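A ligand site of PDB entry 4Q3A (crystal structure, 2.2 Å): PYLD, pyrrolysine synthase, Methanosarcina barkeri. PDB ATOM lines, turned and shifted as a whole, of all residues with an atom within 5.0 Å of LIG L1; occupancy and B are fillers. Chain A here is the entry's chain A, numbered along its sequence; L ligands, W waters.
Water W1 bridges N1 of LIG L1 (2.7 Å) and OD1 of Asp 106 (2.7 Å). Water W5 lies within hydrogen-bond range of O of Val 52 (2.6 Å), O1 of LIG L1 (2.9 Å) and N of Ala 104 (3.0 Å). Water W3 lies within hydrogen-bond range of OD1 of Asn 122 (2.7 Å) and N3 of LIG L1 (3.3 Å). Water W2 lies within hydrogen-bond range of the backbone carbonyl oxygen (O) of Asp 105 (2.8 Å) and a nitrogen (N2) of LIG L1 (3.0 Å).
Leu 4 touches LIG L1. Pro 53 touches LIG L1 (CA to O1, 3.7 Å). CA of Ile 60 touches O2 of LIG L1 (3.4 Å). Phe 64 touches LIG L1. Asp 105 touches LIG L1. Phe 109 touches LIG L1. Asn 122 touches LIG L1. Pro 247 touches LIG L1 (O to C10, 3.7 Å). Hydrophobic or aromatic side chains within 4 Å of LIG L1: Leu 4, Leu 5, Val 54, Ile 60, Ile 61, Phe 64 and Phe 109. 13 residues have an atom within 4 Å of LIG L1: Leu 4, Leu 5, Pro 53, Val 54, Gly 59, Ile 60, Ile 61, Phe 64, Ala 104, Asp 105, Phe 109, Asn 122 and Pro 247.
The backbone carbonyl oxygen of Phe 109 lies within hydrogen-bond range of the backbone NH of Asn 122.
O13 of LG2 L2 lies within hydrogen-bond range of O of Ala 3. N of Val 54 lies within hydrogen-bond range of O1 of LIG L1 (3.0 Å). O2 of LIG L1 sits at hydrogen-bond distance from N of Ile 61, 2.9 Å away. The backbone carbonyl oxygen of Val 54 lies within hydrogen-bond range of a nitrogen (N1) of LIG L1 (2.9 Å). The backbone carbonyl oxygen (O) of Ile 227 lies within hydrogen-bond range of an oxygen (O12) of LG2 L2 (3.5 Å). The backbone carbonyl oxygen (O) of Gly 59 sits close to a nitrogen (N1) of LIG L1, 3.4 Å away. The backbone carbonyl oxygen (O) of Pro 247 lies close to a nitrogen (N7) of LG2 L2 (3.4 Å). O of Ala 104 lies within hydrogen-bond range of N1 of LIG L1 (2.9 Å). The backbone NH (N) of Leu 5 sits at hydrogen-bond distance from an oxygen (O3) of LIG L1 (2.9 Å).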
ATOM      1  N   ALA A   3      25.996 -19.388  12.049  1.00  0.00           N
ATOM      2  CA  ALA A   3      25.537 -18.425  11.045  1.00  0.00           C
ATOM      3  C   ALA A   3      25.700 -16.971  11.498  1.00  0.00           C
ATOM      4  O   ALA A   3      24.751 -16.360  12.034  1.00  0.00           O
ATOM      5  CB  ALA A   3      24.084 -18.709  10.689  1.00  0.00           C
ATOM      6  N   LEU A   4      26.894 -16.427  11.247  1.00  0.00           N
ATOM      7  CA  LEU A   4      27.213 -15.042  11.635  1.00  0.00           C
ATOM      8  C   LEU A   4      27.242 -14.053  10.468  1.00  0.00           C
ATOM      9  O   LEU A   4      27.690 -14.378   9.364  1.00  0.00           O
ATOM     10  CB  LEU A   4      28.570 -14.987  12.345  1.00  0.00           C
ATOM     11  CG  LEU A   4      28.750 -15.902  13.569  1.00  0.00           C
ATOM     12  CD1 LEU A   4      30.052 -15.566  14.244  1.00  0.00           C
ATOM     13  CD2 LEU A   4      27.594 -15.771  14.548  1.00  0.00           C
ATOM     14  N   LEU A   5      26.790 -12.827  10.726  1.00  0.00           N
ATOM     15  CA  LEU A   5      26.848 -11.747   9.742  1.00  0.00           C
ATOM     16  C   LEU A   5      28.261 -11.546   9.234  1.00  0.00           C
ATOM     17  O   LEU A   5      29.241 -11.753   9.962  1.00  0.00           O
ATOM     18  CB  LEU A   5      26.389 -10.433  10.360  1.00  0.00           C
ATOM     19  CG  LEU A   5      24.915 -10.321  10.744  1.00  0.00           C
ATOM     20  CD1 LEU A   5      24.693  -9.129  11.652  1.00  0.00           C
ATOM     21  CD2 LEU A   5      24.032 -10.203   9.521  1.00  0.00           C
ATOM     22  N   VAL A  52      27.992  -1.937  23.016  1.00  0.00           N
ATOM     23  CA  VAL A  52      29.304  -2.389  23.441  1.00  0.00           C
ATOM     24  C   VAL A  52      29.896  -3.395  22.437  1.00  0.00           C
ATOM     25  O   VAL A  52      29.435  -4.530  22.330  1.00  0.00           O
ATOM     26  CB  VAL A  52      29.248  -3.060  24.845  1.00  0.00           C
ATOM     27  CG1 VAL A  52      30.640  -3.524  25.285  1.00  0.00           C
ATOM     28  CG2 VAL A  52      28.653  -2.105  25.878  1.00  0.00           C
ATOM     29  N   PRO A  53      30.962  -2.999  21.715  1.00  0.00           N
ATOM     30  CA  PRO A  53      31.637  -3.993  20.870  1.00  0.00           C
ATOM     31  C   PRO A  53      32.239  -5.110  21.726  1.00  0.00           C
ATOM     32  O   PRO A  53      32.698  -4.850  22.830  1.00  0.00           O
ATOM     33  CB  PRO A  53      32.759  -3.194  20.188  1.00  0.00           C
ATOM     34  CG  PRO A  53      32.357  -1.760  20.347  1.00  0.00           C
ATOM     35  CD  PRO A  53      31.662  -1.704  21.676  1.00  0.00           C
ATOM     36  N   VAL A  54      32.235  -6.323  21.188  1.00  0.00           N
ATOM     37  CA  VAL A  54      32.711  -7.501  21.890  1.00  0.00           C
ATOM     38  C   VAL A  54      33.688  -8.291  20.986  1.00  0.00           C
ATOM     39  O   VAL A  54      33.374  -8.625  19.844  1.00  0.00           O
ATOM     40  CB  VAL A  54      31.512  -8.370  22.305  1.00  0.00           C
ATOM     41  CG1 VAL A  54      31.935  -9.784  22.690  1.00  0.00           C
ATOM     42  CG2 VAL A  54      30.780  -7.713  23.478  1.00  0.00           C
ATOM     43  N   GLY A  59      34.935 -12.442  17.098  1.00  0.00           N
ATOM     44  CA  GLY A  59      35.378 -11.072  17.355  1.00  0.00           C
ATOM     45  C   GLY A  59      34.477 -10.014  16.777  1.00  0.00           C
ATOM     46  O   GLY A  59      33.340 -10.279  16.427  1.00  0.00           O
ATOM     47  N   ILE A  60      34.997  -8.787  16.738  1.00  0.00           N
ATOM     48  CA  ILE A  60      34.266  -7.654  16.218  1.00  0.00           C
ATOM     49  C   ILE A  60      33.944  -7.895  14.749  1.00  0.00           C
ATOM     50  O   ILE A  60      34.832  -8.216  13.969  1.00  0.00           O
ATOM     51  CB  ILE A  60      35.038  -6.337  16.413  1.00  0.00           C
ATOM     52  CG1 ILE A  60      34.946  -5.916  17.886  1.00  0.00           C
ATOM     53  CG2 ILE A  60      34.476  -5.237  15.530  1.00  0.00           C
ATOM     54  CD1 ILE A  60      35.882  -4.801  18.289  1.00  0.00           C
ATOM     55  N   ILE A  61      32.676  -7.796  14.388  1.00  0.00           N
ATOM     56  CA  ILE A  61      32.258  -7.876  12.977  1.00  0.00           C
ATOM     57  C   ILE A  61      32.172  -6.464  12.411  1.00  0.00           C
ATOM     58  O   ILE A  61      31.532  -5.603  13.008  1.00  0.00           O
ATOM     59  CB  ILE A  61      30.896  -8.608  12.818  1.00  0.00           C
ATOM     60  CG1 ILE A  61      31.027 -10.072  13.255  1.00  0.00           C
ATOM     61  CG2 ILE A  61      30.394  -8.526  11.387  1.00  0.00           C
ATOM     62  CD1 ILE A  61      29.710 -10.825  13.295  1.00  0.00           C
ATOM     63  N   PHE A  64      29.024  -3.909  12.327  1.00  0.00           N
ATOM     64  CA  PHE A  64      28.047  -4.370  13.305  1.00  0.00           C
ATOM     65  C   PHE A  64      27.643  -3.276  14.307  1.00  0.00           C
ATOM     66  O   PHE A  64      26.459  -2.989  14.461  1.00  0.00           O
ATOM     67  CB  PHE A  64      28.546  -5.639  14.024  1.00  0.00           C
ATOM     68  CG  PHE A  64      27.534  -6.217  14.967  1.00  0.00           C
ATOM     69  CD1 PHE A  64      26.497  -7.019  14.478  1.00  0.00           C
ATOM     70  CD2 PHE A  64      27.561  -5.915  16.313  1.00  0.00           C
ATOM     71  CE1 PHE A  64      25.528  -7.526  15.343  1.00  0.00           C
ATOM     72  CE2 PHE A  64      26.592  -6.422  17.178  1.00  0.00           C
ATOM     73  CZ  PHE A  64      25.585  -7.221  16.694  1.00  0.00           C
ATOM     74  N   SER A  65      28.609  -2.675  14.995  1.00  0.00           N
ATOM     75  CA  SER A  65      28.279  -1.630  15.988  1.00  0.00           C
ATOM     76  C   SER A  65      27.762  -0.368  15.283  1.00  0.00           C
ATOM     77  O   SER A  65      26.779   0.243  15.729  1.00  0.00           O
ATOM     78  CB  SER A  65      29.466  -1.317  16.891  1.00  0.00           C
ATOM     79  OG  SER A  65      30.521  -0.706  16.149  1.00  0.00           O
ATOM     80  N   ALA A 104      26.637  -8.327  21.880  1.00  0.00           N
ATOM     81  CA  ALA A 104      26.541  -9.677  21.327  1.00  0.00           C
ATOM     82  C   ALA A 104      27.882 -10.366  21.251  1.00  0.00           C
ATOM     83  O   ALA A 104      28.875  -9.761  20.845  1.00  0.00           O
ATOM     84  CB  ALA A 104      25.948  -9.624  19.931  1.00  0.00           C
ATOM     85  N   ASP A 105      27.901 -11.638  21.622  1.00  0.00           N
ATOM     86  CA  ASP A 105      29.012 -12.505  21.268  1.00  0.00           C
ATOM     87  C   ASP A 105      28.537 -13.453  20.161  1.00  0.00           C
ATOM     88  O   ASP A 105      27.466 -13.246  19.604  1.00  0.00           O
ATOM     89  CB  ASP A 105      29.641 -13.205  22.518  1.00  0.00           C
ATOM     90  CG  ASP A 105      28.727 -14.182  23.229  1.00  0.00           C
ATOM     91  OD1 ASP A 105      27.689 -14.630  22.664  1.00  0.00           O
ATOM     92  OD2 ASP A 105      29.066 -14.537  24.392  1.00  0.00           O
ATOM     93  N   ASP A 106      29.317 -14.472  19.825  1.00  0.00           N
ATOM     94  CA  ASP A 106      28.972 -15.356  18.720  1.00  0.00           C
ATOM     95  C   ASP A 106      27.683 -16.152  18.949  1.00  0.00           C
ATOM     96  O   ASP A 106      27.089 -16.599  17.975  1.00  0.00           O
ATOM     97  CB  ASP A 106      30.103 -16.316  18.419  1.00  0.00           C
ATOM     98  CG  ASP A 106      31.353 -15.615  17.918  1.00  0.00           C
ATOM     99  OD1 ASP A 106      31.368 -14.376  17.678  1.00  0.00           O
ATOM    100  OD2 ASP A 106      32.364 -16.329  17.759  1.00  0.00           O
ATOM    101  N   PHE A 109      23.057 -12.371  21.421  1.00  0.00           N
ATOM    102  CA  PHE A 109      22.904 -10.938  21.225  1.00  0.00           C
ATOM    103  C   PHE A 109      21.743 -10.556  22.130  1.00  0.00           C
ATOM    104  O   PHE A 109      20.629 -11.079  21.984  1.00  0.00           O
ATOM    105  CB  PHE A 109      22.627 -10.662  19.741  1.00  0.00           C
ATOM    106  CG  PHE A 109      22.267  -9.214  19.410  1.00  0.00           C
ATOM    107  CD1 PHE A 109      22.706  -8.157  20.198  1.00  0.00           C
ATOM    108  CD2 PHE A 109      21.505  -8.924  18.282  1.00  0.00           C
ATOM    109  CE1 PHE A 109      22.379  -6.837  19.865  1.00  0.00           C
ATOM    110  CE2 PHE A 109      21.188  -7.619  17.936  1.00  0.00           C
ATOM    111  CZ  PHE A 109      21.622  -6.565  18.736  1.00  0.00           C
ATOM    112  N   ASN A 122      18.038 -11.859  21.152  1.00  0.00           N
ATOM    113  CA  ASN A 122      17.763 -11.659  19.740  1.00  0.00           C
ATOM    114  C   ASN A 122      17.000 -12.796  19.033  1.00  0.00           C
ATOM    115  O   ASN A 122      16.193 -12.538  18.128  1.00  0.00           O
ATOM    116  CB  ASN A 122      19.086 -11.395  19.014  1.00  0.00           C
ATOM    117  CG  ASN A 122      18.917 -11.183  17.524  1.00  0.00           C
ATOM    118  OD1 ASN A 122      19.269 -12.056  16.724  1.00  0.00           O
ATOM    119  ND2 ASN A 122      18.386 -10.039  17.148  1.00  0.00           N
ATOM    120  N   ILE A 227      19.365 -15.797   6.352  1.00  0.00           N
ATOM    121  CA  ILE A 227      20.413 -15.224   5.507  1.00  0.00           C
ATOM    122  C   ILE A 227      21.282 -16.368   4.961  1.00  0.00           C
ATOM    123  O   ILE A 227      21.723 -17.221   5.730  1.00  0.00           O
ATOM    124  CB  ILE A 227      21.306 -14.247   6.324  1.00  0.00           C
ATOM    125  CG1 ILE A 227      20.468 -13.136   6.977  1.00  0.00           C
ATOM    126  CG2 ILE A 227      22.381 -13.634   5.435  1.00  0.00           C
ATOM    127  CD1 ILE A 227      21.151 -12.429   8.133  1.00  0.00           C
ATOM    128  N   PRO A 247      18.632  -7.877   7.580  1.00  0.00           N
ATOM    129  CA  PRO A 247      19.649  -8.649   8.325  1.00  0.00           C
ATOM    130  C   PRO A 247      19.827  -8.412   9.828  1.00  0.00           C
ATOM    131  O   PRO A 247      20.476  -9.232  10.486  1.00  0.00           O
ATOM    132  CB  PRO A 247      20.949  -8.313   7.594  1.00  0.00           C
ATOM    133  CG  PRO A 247      20.715  -6.958   7.012  1.00  0.00           C
ATOM    134  CD  PRO A 247      19.260  -6.899   6.661  1.00  0.00           C
ATOM    135  N   LEU A 248      19.257  -7.334  10.390  1.00  0.00           N
ATOM    136  CA  LEU A 248      19.561  -7.011  11.797  1.00  0.00           C
ATOM    137  C   LEU A 248      18.581  -6.054  12.490  1.00  0.00           C
ATOM    138  O   LEU A 248      18.311  -6.217  13.681  1.00  0.00           O
ATOM    139  CB  LEU A 248      20.982  -6.420  11.886  1.00  0.00           C
ATOM    140  CG  LEU A 248      21.582  -6.082  13.252  1.00  0.00           C
ATOM    141  CD1 LEU A 248      21.752  -7.315  14.123  1.00  0.00           C
ATOM    142  CD2 LEU A 248      22.916  -5.354  13.098  1.00  0.00           C
HETATM  143  O1  LIG L   1      30.613  -6.859  18.726  1.00  0.00           O
HETATM  144  C1  LIG L   1      30.740  -7.398  17.617  1.00  0.00           C
HETATM  145  O2  LIG L   1      31.069  -6.661  16.550  1.00  0.00           O
HETATM  146  C2  LIG L   1      30.522  -8.878  17.447  1.00  0.00           C
HETATM  147  N1  LIG L   1      30.843  -9.580  18.673  1.00  0.00           N
HETATM  148  C3  LIG L   1      29.077  -9.152  17.057  1.00  0.00           C
HETATM  149  C4  LIG L   1      28.776 -10.636  16.937  1.00  0.00           C
HETATM  150  C5  LIG L   1      27.384 -10.849  16.394  1.00  0.00           C
HETATM  151  C6  LIG L   1      27.136 -12.297  16.001  1.00  0.00           C
HETATM  152  N2  LIG L   1      25.738 -12.567  15.700  1.00  0.00           N
HETATM  153  C7  LIG L   1      25.307 -12.574  14.437  1.00  0.00           C
HETATM  154  O3  LIG L   1      26.057 -12.373  13.492  1.00  0.00           O
HETATM  155  C8  LIG L   1      23.841 -12.825  14.173  1.00  0.00           C
HETATM  156  C9  LIG L   1      23.100 -11.516  13.912  1.00  0.00           C
HETATM  157  C10 LIG L   1      22.067 -11.643  12.795  1.00  0.00           C
HETATM  158  C11 LIG L   1      22.457 -11.110  15.231  1.00  0.00           C
HETATM  159  C12 LIG L   1      22.480 -12.429  15.950  1.00  0.00           C
HETATM  160  N3  LIG L   1      23.151 -13.322  15.345  1.00  0.00           N
HETATM  161  P1  LG2 L   2      19.592 -22.512  13.928  1.00  0.00           P
HETATM  162  O1  LG2 L   2      20.812 -23.254  13.447  1.00  0.00           O
HETATM  163  O2  LG2 L   2      19.175 -22.516  15.373  1.00  0.00           O
HETATM  164  O3  LG2 L   2      18.296 -23.015  13.117  1.00  0.00           O
HETATM  165  C1  LG2 L   2      18.255 -23.063  11.702  1.00  0.00           C
HETATM  166  C2  LG2 L   2      17.413 -24.253  11.316  1.00  0.00           C
HETATM  167  O4  LG2 L   2      17.188 -24.304   9.912  1.00  0.00           O
HETATM  168  C3  LG2 L   2      18.088 -25.565  11.713  1.00  0.00           C
HETATM  169  O5  LG2 L   2      17.237 -26.296  12.593  1.00  0.00           O
HETATM  170  C4  LG2 L   2      18.258 -26.348  10.439  1.00  0.00           C
HETATM  171  O6  LG2 L   2      17.963 -27.731  10.633  1.00  0.00           O
HETATM  172  C5  LG2 L   2      17.224 -25.676   9.539  1.00  0.00           C
HETATM  173  N1  LG2 L   2      17.554 -25.834   8.122  1.00  0.00           N
HETATM  174  C6  LG2 L   2      18.757 -25.681   7.536  1.00  0.00           C
HETATM  175  N2  LG2 L   2      18.667 -25.895   6.212  1.00  0.00           N
HETATM  176  C7  LG2 L   2      17.386 -26.196   5.937  1.00  0.00           C
HETATM  177  C8  LG2 L   2      16.604 -26.552   4.749  1.00  0.00           C
HETATM  178  N3  LG2 L   2      17.208 -26.600   3.547  1.00  0.00           N
HETATM  179  N4  LG2 L   2      15.285 -26.785   4.895  1.00  0.00           N
HETATM  180  C9  LG2 L   2      14.676 -26.720   6.098  1.00  0.00           C
HETATM  181  N5  LG2 L   2      15.328 -26.426   7.223  1.00  0.00           N
HETATM  182  C10 LG2 L   2      16.650 -26.151   7.209  1.00  0.00           C
HETATM  183  O7  LG2 L   2      19.775 -21.003  13.441  1.00  0.00           O
HETATM  184  P2  LG2 L   2      18.938 -19.774  14.038  1.00  0.00           P
HETATM  185  O8  LG2 L   2      19.622 -19.163  15.200  1.00  0.00           O
HETATM  186  O9  LG2 L   2      17.473 -20.181  14.134  1.00  0.00           O
HETATM  187  O10 LG2 L   2      19.132 -18.737  12.823  1.00  0.00           O
HETATM  188  C11 LG2 L   2      18.474 -18.918  11.577  1.00  0.00           C
HETATM  189  C12 LG2 L   2      18.936 -17.871  10.572  1.00  0.00           C
HETATM  190  O11 LG2 L   2      18.484 -16.586  10.986  1.00  0.00           O
HETATM  191  C13 LG2 L   2      20.449 -17.754  10.429  1.00  0.00           C
HETATM  192  O12 LG2 L   2      20.783 -17.585   9.041  1.00  0.00           O
HETATM  193  C14 LG2 L   2      20.798 -16.488  11.193  1.00  0.00           C
HETATM  194  O13 LG2 L   2      21.956 -15.827  10.694  1.00  0.00           O
HETATM  195  C15 LG2 L   2      19.568 -15.654  10.899  1.00  0.00           C
HETATM  196  N6  LG2 L   2      19.254 -14.584  11.841  1.00  0.00           N
HETATM  197  C16 LG2 L   2      18.828 -13.425  11.325  1.00  0.00           C
HETATM  198  C17 LG2 L   2      18.472 -12.348  12.120  1.00  0.00           C
HETATM  199  C18 LG2 L   2      17.955 -11.064  11.481  1.00  0.00           C
HETATM  200  O14 LG2 L   2      17.738 -10.071  12.155  1.00  0.00           O
HETATM  201  N7  LG2 L   2      17.637 -11.059  10.188  1.00  0.00           N
HETATM  202  C19 LG2 L   2      18.538 -12.465  13.624  1.00  0.00           C
HETATM  203  C20 LG2 L   2      18.995 -13.775  14.072  1.00  0.00           C
HETATM  204  C21 LG2 L   2      19.330 -14.775  13.174  1.00  0.00           C
HETATM  205  O   HOH W   1      31.610 -12.130  19.197  1.00  0.00           O
HETATM  206  O   HOH W   2      24.853 -13.111  18.492  1.00  0.00           O
HETATM  207  O   HOH W   3      20.655 -14.374  17.176  1.00  0.00           O
HETATM  208  O   HOH W   4      31.122  -4.130  17.048  1.00  0.00           O
HETATM  209  O   HOH W   5      28.507  -6.306  20.617  1.00  0.00           O
HETATM  210  O   HOH W   6      23.305 -15.813  15.765  1.00  0.00           O
